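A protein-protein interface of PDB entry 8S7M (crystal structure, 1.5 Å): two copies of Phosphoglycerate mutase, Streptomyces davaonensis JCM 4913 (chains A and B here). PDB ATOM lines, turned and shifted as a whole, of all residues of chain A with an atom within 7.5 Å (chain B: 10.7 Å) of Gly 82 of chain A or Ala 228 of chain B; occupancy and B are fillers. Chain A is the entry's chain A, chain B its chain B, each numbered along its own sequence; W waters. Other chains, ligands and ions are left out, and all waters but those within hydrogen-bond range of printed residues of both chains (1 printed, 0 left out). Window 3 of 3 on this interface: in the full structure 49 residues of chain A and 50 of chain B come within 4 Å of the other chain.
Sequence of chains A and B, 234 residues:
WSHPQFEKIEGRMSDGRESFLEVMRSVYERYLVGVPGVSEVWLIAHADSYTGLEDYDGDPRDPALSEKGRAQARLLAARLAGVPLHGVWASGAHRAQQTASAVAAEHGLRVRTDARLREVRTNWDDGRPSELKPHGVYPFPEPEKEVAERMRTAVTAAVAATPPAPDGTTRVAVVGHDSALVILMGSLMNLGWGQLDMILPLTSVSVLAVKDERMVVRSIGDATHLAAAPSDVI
Water W1 lies within hydrogen-bond range of NE of Arg 79 of chain A (3.0 Å) and OG1 of Thr 224 of chain B (3.1 Å).
CH2 of Trp 42 of chain A touches CG2 of Thr 224 of chain B (3.6 Å).
Ala 227 of chain B touches Trp 42 of chain A (CB to CZ2, 3.8 Å).
Gly 82 of chain A touches Ala 228 of chain B.
Ala 228 of chain B touches Pro 84 of chain A.
No position is printed for both chains.
Of the 7 pairs that touch across the chains among the printed residues, none has its exchanged pair printed and touching as well.
The backbone carbonyl oxygen (O) of Pro 84 of chain A sits at hydrogen-bond distance from the guanidinium group (NH1) of Arg 171 of chain A (2.9 Å).
The side-chain hydroxyl (OG1) of Thr 224 of chain B sits at hydrogen-bond distance from the side-chain carboxylate (OD1) of Asp 222 of chain B, at 2.6 Å.
Of chain B, only Ala 228 (3.6 Å) comes within 4 Å of Gly 82 of chain A.
Ala 228 of chain B touches just these residues of chain A: Gly 82 (3.6 Å) and Pro 84 (3.96 Å).
Of the printed residues of chain B, Pro 84 of chain A touches Ala 228 (3.96 Å).
Ala 227 of chain B touches just these residues of chain A: Trp 42 and Arg 171.
Printed residues of chain A within 4 Å of Asp 222 of chain B: Arg 79.
Of the printed residues of chain B, Arg 79 of chain A touches Asp 222 and Thr 224.
The nearest residue of chain B that does not touch Gly 82 of chain A is Ala 227 of chain B (6.1 Å).
The nearest printed residue of chain A that does not touch Thr 224 of chain B is Val 83 of chain A (5.1 Å).
Of the 15 printed residues of chain B, 4 touch a printed residue of chain A.
Hydrophobic or aromatic side chains of chain B that line the printed part of chain A: Ala 227 and Ala 228.
Of the 13 printed residues of chain A, 5 touch a printed residue of chain B.
Hydrophobic or aromatic side chains of chain A within 4 Å of the printed part of chain B: Trp 42 and Pro 84.
Among the printed residues, 7 pairs touch across the chains.
NH2 of Arg 79 of chain A lies within salt-bridge range of OD2 of Asp 222 of chain B (3.0 Å).
The side-chain hydroxyl of Thr 224 of chain B lies within hydrogen-bond range of the guanidinium group of Arg 79 of chain A, at 3.0 Å.
NH2 of Arg 171 of chain A sits at hydrogen-bond distance from O of Ala 227 of chain B (3.4 Å).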
ATOM      1  N   TRP A  42      -7.394 -31.886  19.596  1.00  0.00           N
ATOM      2  CA  TRP A  42      -7.790 -30.523  19.261  1.00  0.00           C
ATOM      3  C   TRP A  42      -9.303 -30.450  19.389  1.00  0.00           C
ATOM      4  O   TRP A  42     -10.040 -30.960  18.530  1.00  0.00           O
ATOM      5  CB  TRP A  42      -7.292 -30.100  17.887  1.00  0.00           C
ATOM      6  CG  TRP A  42      -5.816 -29.852  17.884  1.00  0.00           C
ATOM      7  CD1 TRP A  42      -4.875 -30.449  18.680  1.00  0.00           C
ATOM      8  CD2 TRP A  42      -5.107 -28.930  17.048  1.00  0.00           C
ATOM      9  NE1 TRP A  42      -3.611 -29.954  18.380  1.00  0.00           N
ATOM     10  CE2 TRP A  42      -3.739 -29.007  17.399  1.00  0.00           C
ATOM     11  CE3 TRP A  42      -5.501 -28.034  16.053  1.00  0.00           C
ATOM     12  CZ2 TRP A  42      -2.768 -28.240  16.768  1.00  0.00           C
ATOM     13  CZ3 TRP A  42      -4.529 -27.256  15.438  1.00  0.00           C
ATOM     14  CH2 TRP A  42      -3.182 -27.381  15.792  1.00  0.00           C
ATOM     15  N   ALA A  77     -10.898 -24.504   8.455  1.00  0.00           N
ATOM     16  CA  ALA A  77     -10.318 -25.562   7.640  1.00  0.00           C
ATOM     17  C   ALA A  77      -8.989 -25.121   7.043  1.00  0.00           C
ATOM     18  O   ALA A  77      -8.047 -25.919   6.968  1.00  0.00           O
ATOM     19  CB  ALA A  77     -11.296 -25.988   6.537  1.00  0.00           C
ATOM     20  N   ALA A  78      -8.898 -23.857   6.605  1.00  0.00           N
ATOM     21  CA  ALA A  78      -7.643 -23.361   6.044  1.00  0.00           C
ATOM     22  C   ALA A  78      -6.553 -23.331   7.102  1.00  0.00           C
ATOM     23  O   ALA A  78      -5.390 -23.666   6.815  1.00  0.00           O
ATOM     24  CB  ALA A  78      -7.841 -21.973   5.424  1.00  0.00           C
ATOM     25  N   ARG A  79      -6.917 -22.978   8.341  1.00  0.00           N
ATOM     26  CA  ARG A  79      -5.955 -22.996   9.434  1.00  0.00           C
ATOM     27  C   ARG A  79      -5.427 -24.399   9.689  1.00  0.00           C
ATOM     28  O   ARG A  79      -4.229 -24.585   9.925  1.00  0.00           O
ATOM     29  CB  ARG A  79      -6.611 -22.437  10.694  1.00  0.00           C
ATOM     30  CG  ARG A  79      -5.753 -22.572  11.941  1.00  0.00           C
ATOM     31  CD  ARG A  79      -6.505 -22.138  13.175  1.00  0.00           C
ATOM     32  NE  ARG A  79      -5.736 -22.451  14.375  1.00  0.00           N
ATOM     33  CZ  ARG A  79      -6.021 -21.995  15.586  1.00  0.00           C
ATOM     34  NH1 ARG A  79      -7.104 -21.263  15.809  1.00  0.00           N
ATOM     35  NH2 ARG A  79      -5.205 -22.284  16.596  1.00  0.00           N
ATOM     36  N   LEU A  80      -6.301 -25.396   9.653  1.00  0.00           N
ATOM     37  CA  LEU A  80      -5.910 -26.760   9.968  1.00  0.00           C
ATOM     38  C   LEU A  80      -5.358 -27.507   8.762  1.00  0.00           C
ATOM     39  O   LEU A  80      -4.887 -28.639   8.923  1.00  0.00           O
ATOM     40  CB  LEU A  80      -7.114 -27.536  10.523  1.00  0.00           C
ATOM     41  CG  LEU A  80      -7.715 -26.981  11.823  1.00  0.00           C
ATOM     42  CD1 LEU A  80      -8.825 -27.870  12.376  1.00  0.00           C
ATOM     43  CD2 LEU A  80      -6.648 -26.789  12.849  1.00  0.00           C
ATOM     44  N   ALA A  81      -5.383 -26.911   7.566  1.00  0.00           N
ATOM     45  CA  ALA A  81      -5.000 -27.687   6.384  1.00  0.00           C
ATOM     46  C   ALA A  81      -3.556 -28.165   6.482  1.00  0.00           C
ATOM     47  O   ALA A  81      -3.235 -29.282   6.060  1.00  0.00           O
ATOM     48  CB  ALA A  81      -5.223 -26.871   5.114  1.00  0.00           C
ATOM     49  N   GLY A  82      -2.681 -27.349   7.061  1.00  0.00           N
ATOM     50  CA  GLY A  82      -1.289 -27.713   7.214  1.00  0.00           C
ATOM     51  C   GLY A  82      -0.955 -28.429   8.494  1.00  0.00           C
ATOM     52  O   GLY A  82       0.217 -28.751   8.732  1.00  0.00           O
ATOM     53  N   VAL A  83      -1.948 -28.698   9.332  1.00  0.00           N
ATOM     54  CA  VAL A  83      -1.737 -29.368  10.611  1.00  0.00           C
ATOM     55  C   VAL A  83      -2.007 -30.855  10.401  1.00  0.00           C
ATOM     56  O   VAL A  83      -3.106 -31.212   9.946  1.00  0.00           O
ATOM     57  CB  VAL A  83      -2.691 -28.810  11.669  1.00  0.00           C
ATOM     58  CG1 VAL A  83      -2.589 -29.603  12.951  1.00  0.00           C
ATOM     59  CG2 VAL A  83      -2.413 -27.330  11.893  1.00  0.00           C
ATOM     60  N   PRO A  84      -1.065 -31.741  10.714  1.00  0.00           N
ATOM     61  CA  PRO A  84      -1.364 -33.181  10.579  1.00  0.00           C
ATOM     62  C   PRO A  84      -2.469 -33.604  11.541  1.00  0.00           C
ATOM     63  O   PRO A  84      -2.449 -33.267  12.728  1.00  0.00           O
ATOM     64  CB  PRO A  84      -0.028 -33.861  10.909  1.00  0.00           C
ATOM     65  CG  PRO A  84       1.012 -32.814  10.626  1.00  0.00           C
ATOM     66  CD  PRO A  84       0.359 -31.488  10.987  1.00  0.00           C
ATOM     67  N   LEU A  85      -3.454 -34.329  11.011  1.00  0.00           N
ATOM     68  CA  LEU A  85      -4.579 -34.835  11.787  1.00  0.00           C
ATOM     69  C   LEU A  85      -4.802 -36.286  11.423  1.00  0.00           C
ATOM     70  O   LEU A  85      -4.792 -36.652  10.243  1.00  0.00           O
ATOM     71  CB  LEU A  85      -5.872 -34.087  11.472  1.00  0.00           C
ATOM     72  CG  LEU A  85      -5.904 -32.620  11.870  1.00  0.00           C
ATOM     73  CD1 LEU A  85      -7.234 -32.044  11.434  1.00  0.00           C
ATOM     74  CD2 LEU A  85      -5.752 -32.514  13.374  1.00  0.00           C
ATOM     75  N   GLU A 106     -10.013 -32.453   3.948  1.00  0.00           N
ATOM     76  CA  GLU A 106      -8.658 -32.038   3.583  1.00  0.00           C
ATOM     77  C   GLU A 106      -7.555 -32.840   4.253  1.00  0.00           C
ATOM     78  O   GLU A 106      -6.375 -32.564   4.014  1.00  0.00           O
ATOM     79  CB  GLU A 106      -8.484 -30.548   3.801  1.00  0.00           C
ATOM     80  CG  GLU A 106      -9.456 -29.796   2.935  1.00  0.00           C
ATOM     81  CD  GLU A 106      -9.719 -28.419   3.430  1.00  0.00           C
ATOM     82  OE1 GLU A 106      -8.976 -27.982   4.333  1.00  0.00           O
ATOM     83  OE2 GLU A 106     -10.679 -27.792   2.922  1.00  0.00           O
ATOM     84  N   HIS A 107      -7.908 -33.837   5.049  1.00  0.00           N
ATOM     85  CA  HIS A 107      -6.938 -34.733   5.660  1.00  0.00           C
ATOM     86  C   HIS A 107      -7.192 -36.180   5.274  1.00  0.00           C
ATOM     87  O   HIS A 107      -6.617 -37.080   5.891  1.00  0.00           O
ATOM     88  CB  HIS A 107      -6.963 -34.569   7.179  1.00  0.00           C
ATOM     89  CG  HIS A 107      -6.493 -33.224   7.626  1.00  0.00           C
ATOM     90  ND1 HIS A 107      -7.315 -32.118   7.650  1.00  0.00           N
ATOM     91  CD2 HIS A 107      -5.267 -32.795   7.997  1.00  0.00           C
ATOM     92  CE1 HIS A 107      -6.618 -31.068   8.058  1.00  0.00           C
ATOM     93  NE2 HIS A 107      -5.372 -31.451   8.268  1.00  0.00           N
ATOM     94  N   ARG A 171      -2.529 -36.673  16.440  1.00  0.00           N
ATOM     95  CA  ARG A 171      -3.476 -35.602  16.720  1.00  0.00           C
ATOM     96  C   ARG A 171      -4.871 -36.011  16.273  1.00  0.00           C
ATOM     97  O   ARG A 171      -5.057 -36.451  15.136  1.00  0.00           O
ATOM     98  CB  ARG A 171      -3.053 -34.333  15.977  1.00  0.00           C
ATOM     99  CG  ARG A 171      -3.785 -33.055  16.363  1.00  0.00           C
ATOM    100  CD  ARG A 171      -3.074 -31.857  15.721  1.00  0.00           C
ATOM    101  NE  ARG A 171      -1.783 -31.575  16.350  1.00  0.00           N
ATOM    102  CZ  ARG A 171      -0.590 -31.748  15.781  1.00  0.00           C
ATOM    103  NH1 ARG A 171      -0.464 -32.183  14.532  1.00  0.00           N
ATOM    104  NH2 ARG A 171       0.510 -31.479  16.480  1.00  0.00           N
ATOM    105  N   ALA B  71      13.951 -19.819  15.262  1.00  0.00           N
ATOM    106  CA  ALA B  71      13.031 -20.557  14.404  1.00  0.00           C
ATOM    107  C   ALA B  71      11.590 -20.457  14.899  1.00  0.00           C
ATOM    108  O   ALA B  71      10.671 -20.291  14.089  1.00  0.00           O
ATOM    109  CB  ALA B  71      13.480 -22.011  14.290  1.00  0.00           C
ATOM    110  N   LEU B  75       8.284 -18.687  12.865  1.00  0.00           N
ATOM    111  CA  LEU B  75       6.951 -19.265  12.697  1.00  0.00           C
ATOM    112  C   LEU B  75       5.873 -18.377  13.300  1.00  0.00           C
ATOM    113  O   LEU B  75       4.816 -18.186  12.698  1.00  0.00           O
ATOM    114  CB  LEU B  75       6.882 -20.666  13.298  1.00  0.00           C
ATOM    115  CG  LEU B  75       7.704 -21.691  12.532  1.00  0.00           C
ATOM    116  CD1 LEU B  75       7.801 -22.971  13.328  1.00  0.00           C
ATOM    117  CD2 LEU B  75       7.092 -21.972  11.165  1.00  0.00           C
ATOM    118  N   ASP B 222      -1.894 -20.658  23.119  1.00  0.00           N
ATOM    119  CA  ASP B 222      -1.930 -21.323  21.823  1.00  0.00           C
ATOM    120  C   ASP B 222      -0.603 -21.153  21.086  1.00  0.00           C
ATOM    121  O   ASP B 222      -0.245 -20.046  20.664  1.00  0.00           O
ATOM    122  CB  ASP B 222      -3.116 -20.792  21.025  1.00  0.00           C
ATOM    123  CG  ASP B 222      -3.246 -21.445  19.676  1.00  0.00           C
ATOM    124  OD1 ASP B 222      -2.262 -21.437  18.891  1.00  0.00           O
ATOM    125  OD2 ASP B 222      -4.293 -22.068  19.436  1.00  0.00           O
ATOM    126  N   ALA B 223       0.113 -22.259  20.903  1.00  0.00           N
ATOM    127  CA  ALA B 223       1.351 -22.261  20.135  1.00  0.00           C
ATOM    128  C   ALA B 223       1.215 -23.139  18.900  1.00  0.00           C
ATOM    129  O   ALA B 223       2.176 -23.802  18.493  1.00  0.00           O
ATOM    130  CB  ALA B 223       2.547 -22.676  20.998  1.00  0.00           C
ATOM    131  N   THR B 224       0.017 -23.135  18.295  1.00  0.00           N
ATOM    132  CA  THR B 224      -0.284 -24.074  17.211  1.00  0.00           C
ATOM    133  C   THR B 224       0.499 -23.801  15.927  1.00  0.00           C
ATOM    134  O   THR B 224       0.540 -24.680  15.050  1.00  0.00           O
ATOM    135  CB  THR B 224      -1.787 -24.148  16.958  1.00  0.00           C
ATOM    136  OG1 THR B 224      -2.273 -22.836  16.650  1.00  0.00           O
ATOM    137  CG2 THR B 224      -2.532 -24.723  18.176  1.00  0.00           C
ATOM    138  N   HIS B 225       1.173 -22.647  15.817  1.00  0.00           N
ATOM    139  CA  HIS B 225       2.081 -22.443  14.696  1.00  0.00           C
ATOM    140  C   HIS B 225       3.262 -23.405  14.735  1.00  0.00           C
ATOM    141  O   HIS B 225       3.976 -23.528  13.733  1.00  0.00           O
ATOM    142  CB  HIS B 225       2.568 -20.986  14.658  1.00  0.00           C
ATOM    143  CG  HIS B 225       3.072 -20.493  15.980  1.00  0.00           C
ATOM    144  ND1 HIS B 225       2.221 -20.063  16.976  1.00  0.00           N
ATOM    145  CD2 HIS B 225       4.325 -20.418  16.488  1.00  0.00           C
ATOM    146  CE1 HIS B 225       2.936 -19.702  18.029  1.00  0.00           C
ATOM    147  NE2 HIS B 225       4.212 -19.921  17.765  1.00  0.00           N
ATOM    148  N   LEU B 226       3.488 -24.079  15.861  1.00  0.00           N
ATOM    149  CA  LEU B 226       4.543 -25.077  15.972  1.00  0.00           C
ATOM    150  C   LEU B 226       4.053 -26.487  15.670  1.00  0.00           C
ATOM    151  O   LEU B 226       4.854 -27.425  15.706  1.00  0.00           O
ATOM    152  CB  LEU B 226       5.169 -25.037  17.371  1.00  0.00           C
ATOM    153  CG  LEU B 226       5.616 -23.650  17.835  1.00  0.00           C
ATOM    154  CD1 LEU B 226       6.213 -23.699  19.247  1.00  0.00           C
ATOM    155  CD2 LEU B 226       6.623 -23.036  16.868  1.00  0.00           C
ATOM    156  N   ALA B 227       2.764 -26.665  15.349  1.00  0.00           N
ATOM    157  CA  ALA B 227       2.187 -28.016  15.311  1.00  0.00           C
ATOM    158  C   ALA B 227       2.806 -28.911  14.249  1.00  0.00           C
ATOM    159  O   ALA B 227       2.807 -30.139  14.410  1.00  0.00           O
ATOM    160  CB  ALA B 227       0.668 -27.956  15.096  1.00  0.00           C
ATOM    161  N   ALA B 228       3.274 -28.347  13.142  1.00  0.00           N
ATOM    162  CA  ALA B 228       3.853 -29.152  12.074  1.00  0.00           C
ATOM    163  C   ALA B 228       5.371 -29.041  12.028  1.00  0.00           C
ATOM    164  O   ALA B 228       6.002 -29.575  11.107  1.00  0.00           O
ATOM    165  CB  ALA B 228       3.230 -28.779  10.728  1.00  0.00           C
ATOM    166  N   ALA B 229       5.966 -28.379  13.006  1.00  0.00           N
ATOM    167  CA  ALA B 229       7.386 -28.101  12.959  1.00  0.00           C
ATOM    168  C   ALA B 229       8.198 -29.316  13.402  1.00  0.00           C
ATOM    169  O   ALA B 229       7.696 -30.192  14.107  1.00  0.00           O
ATOM    170  CB  ALA B 229       7.687 -26.902  13.850  1.00  0.00           C
ATOM    171  N   PRO B 230       9.458 -29.402  12.984  1.00  0.00           N
ATOM    172  CA  PRO B 230      10.325 -30.478  13.471  1.00  0.00           C
ATOM    173  C   PRO B 230      10.497 -30.400  14.980  1.00  0.00           C
ATOM    174  O   PRO B 230      10.311 -29.350  15.602  1.00  0.00           O
ATOM    175  CB  PRO B 230      11.651 -30.206  12.755  1.00  0.00           C
ATOM    176  CG  PRO B 230      11.259 -29.502  11.480  1.00  0.00           C
ATOM    177  CD  PRO B 230      10.079 -28.637  11.885  1.00  0.00           C
ATOM    178  N   SER B 231      10.899 -31.533  15.562  1.00  0.00           N
ATOM    179  CA  SER B 231      10.990 -31.666  17.012  1.00  0.00           C
ATOM    180  C   SER B 231      12.084 -30.799  17.637  1.00  0.00           C
ATOM    181  O   SER B 231      11.962 -30.435  18.812  1.00  0.00           O
ATOM    182  CB  SER B 231      11.176 -33.134  17.399  1.00  0.00           C
ATOM    183  OG  SER B 231      12.442 -33.614  16.981  1.00  0.00           O
ATOM    184  N   ASP B 232      13.146 -30.457  16.898  1.00  0.00           N
ATOM    185  CA  ASP B 232      14.155 -29.547  17.438  1.00  0.00           C
ATOM    186  C   ASP B 232      13.706 -28.082  17.439  1.00  0.00           C
ATOM    187  O   ASP B 232      14.493 -27.207  17.817  1.00  0.00           O
ATOM    188  CB  ASP B 232      15.521 -29.720  16.754  1.00  0.00           C
ATOM    189  CG  ASP B 232      15.475 -29.475  15.255  1.00  0.00           C
ATOM    190  OD1 ASP B 232      14.368 -29.392  14.691  1.00  0.00           O
ATOM    191  OD2 ASP B 232      16.559 -29.374  14.631  1.00  0.00           O
ATOM    192  N   VAL B 233      12.472 -27.810  17.018  1.00  0.00           N
ATOM    193  CA  VAL B 233      11.906 -26.475  17.100  1.00  0.00           C
ATOM    194  C   VAL B 233      10.866 -26.362  18.217  1.00  0.00           C
ATOM    195  O   VAL B 233      10.638 -25.258  18.736  1.00  0.00           O
ATOM    196  CB  VAL B 233      11.311 -26.068  15.729  1.00  0.00           C
ATOM    197  CG1 VAL B 233      10.572 -24.735  15.790  1.00  0.00           C
ATOM    198  CG2 VAL B 233      12.405 -26.027  14.671  1.00  0.00           C
ATOM    199  N   ILE B 234      10.256 -27.470  18.628  1.00  0.00           N
ATOM    200  CA  ILE B 234       9.184 -27.452  19.622  1.00  0.00           C
ATOM    201  C   ILE B 234       9.700 -27.090  21.011  1.00  0.00           C
ATOM    202  O   ILE B 234       9.115 -26.252  21.705  1.00  0.00           O
ATOM    203  CB  ILE B 234       8.408 -28.789  19.624  1.00  0.00           C
ATOM    204  CG1 ILE B 234       7.209 -28.713  18.676  1.00  0.00           C
ATOM    205  CG2 ILE B 234       7.953 -29.149  21.032  1.00  0.00           C
ATOM    206  CD1 ILE B 234       7.576 -28.584  17.224  1.00  0.00           C
ATOM    207  OXT ILE B 234      10.722 -27.610  21.463  1.00  0.00           O
HETATM  208  O   HOH W   1      -3.238 -23.965  13.926  1.00  0.00           O
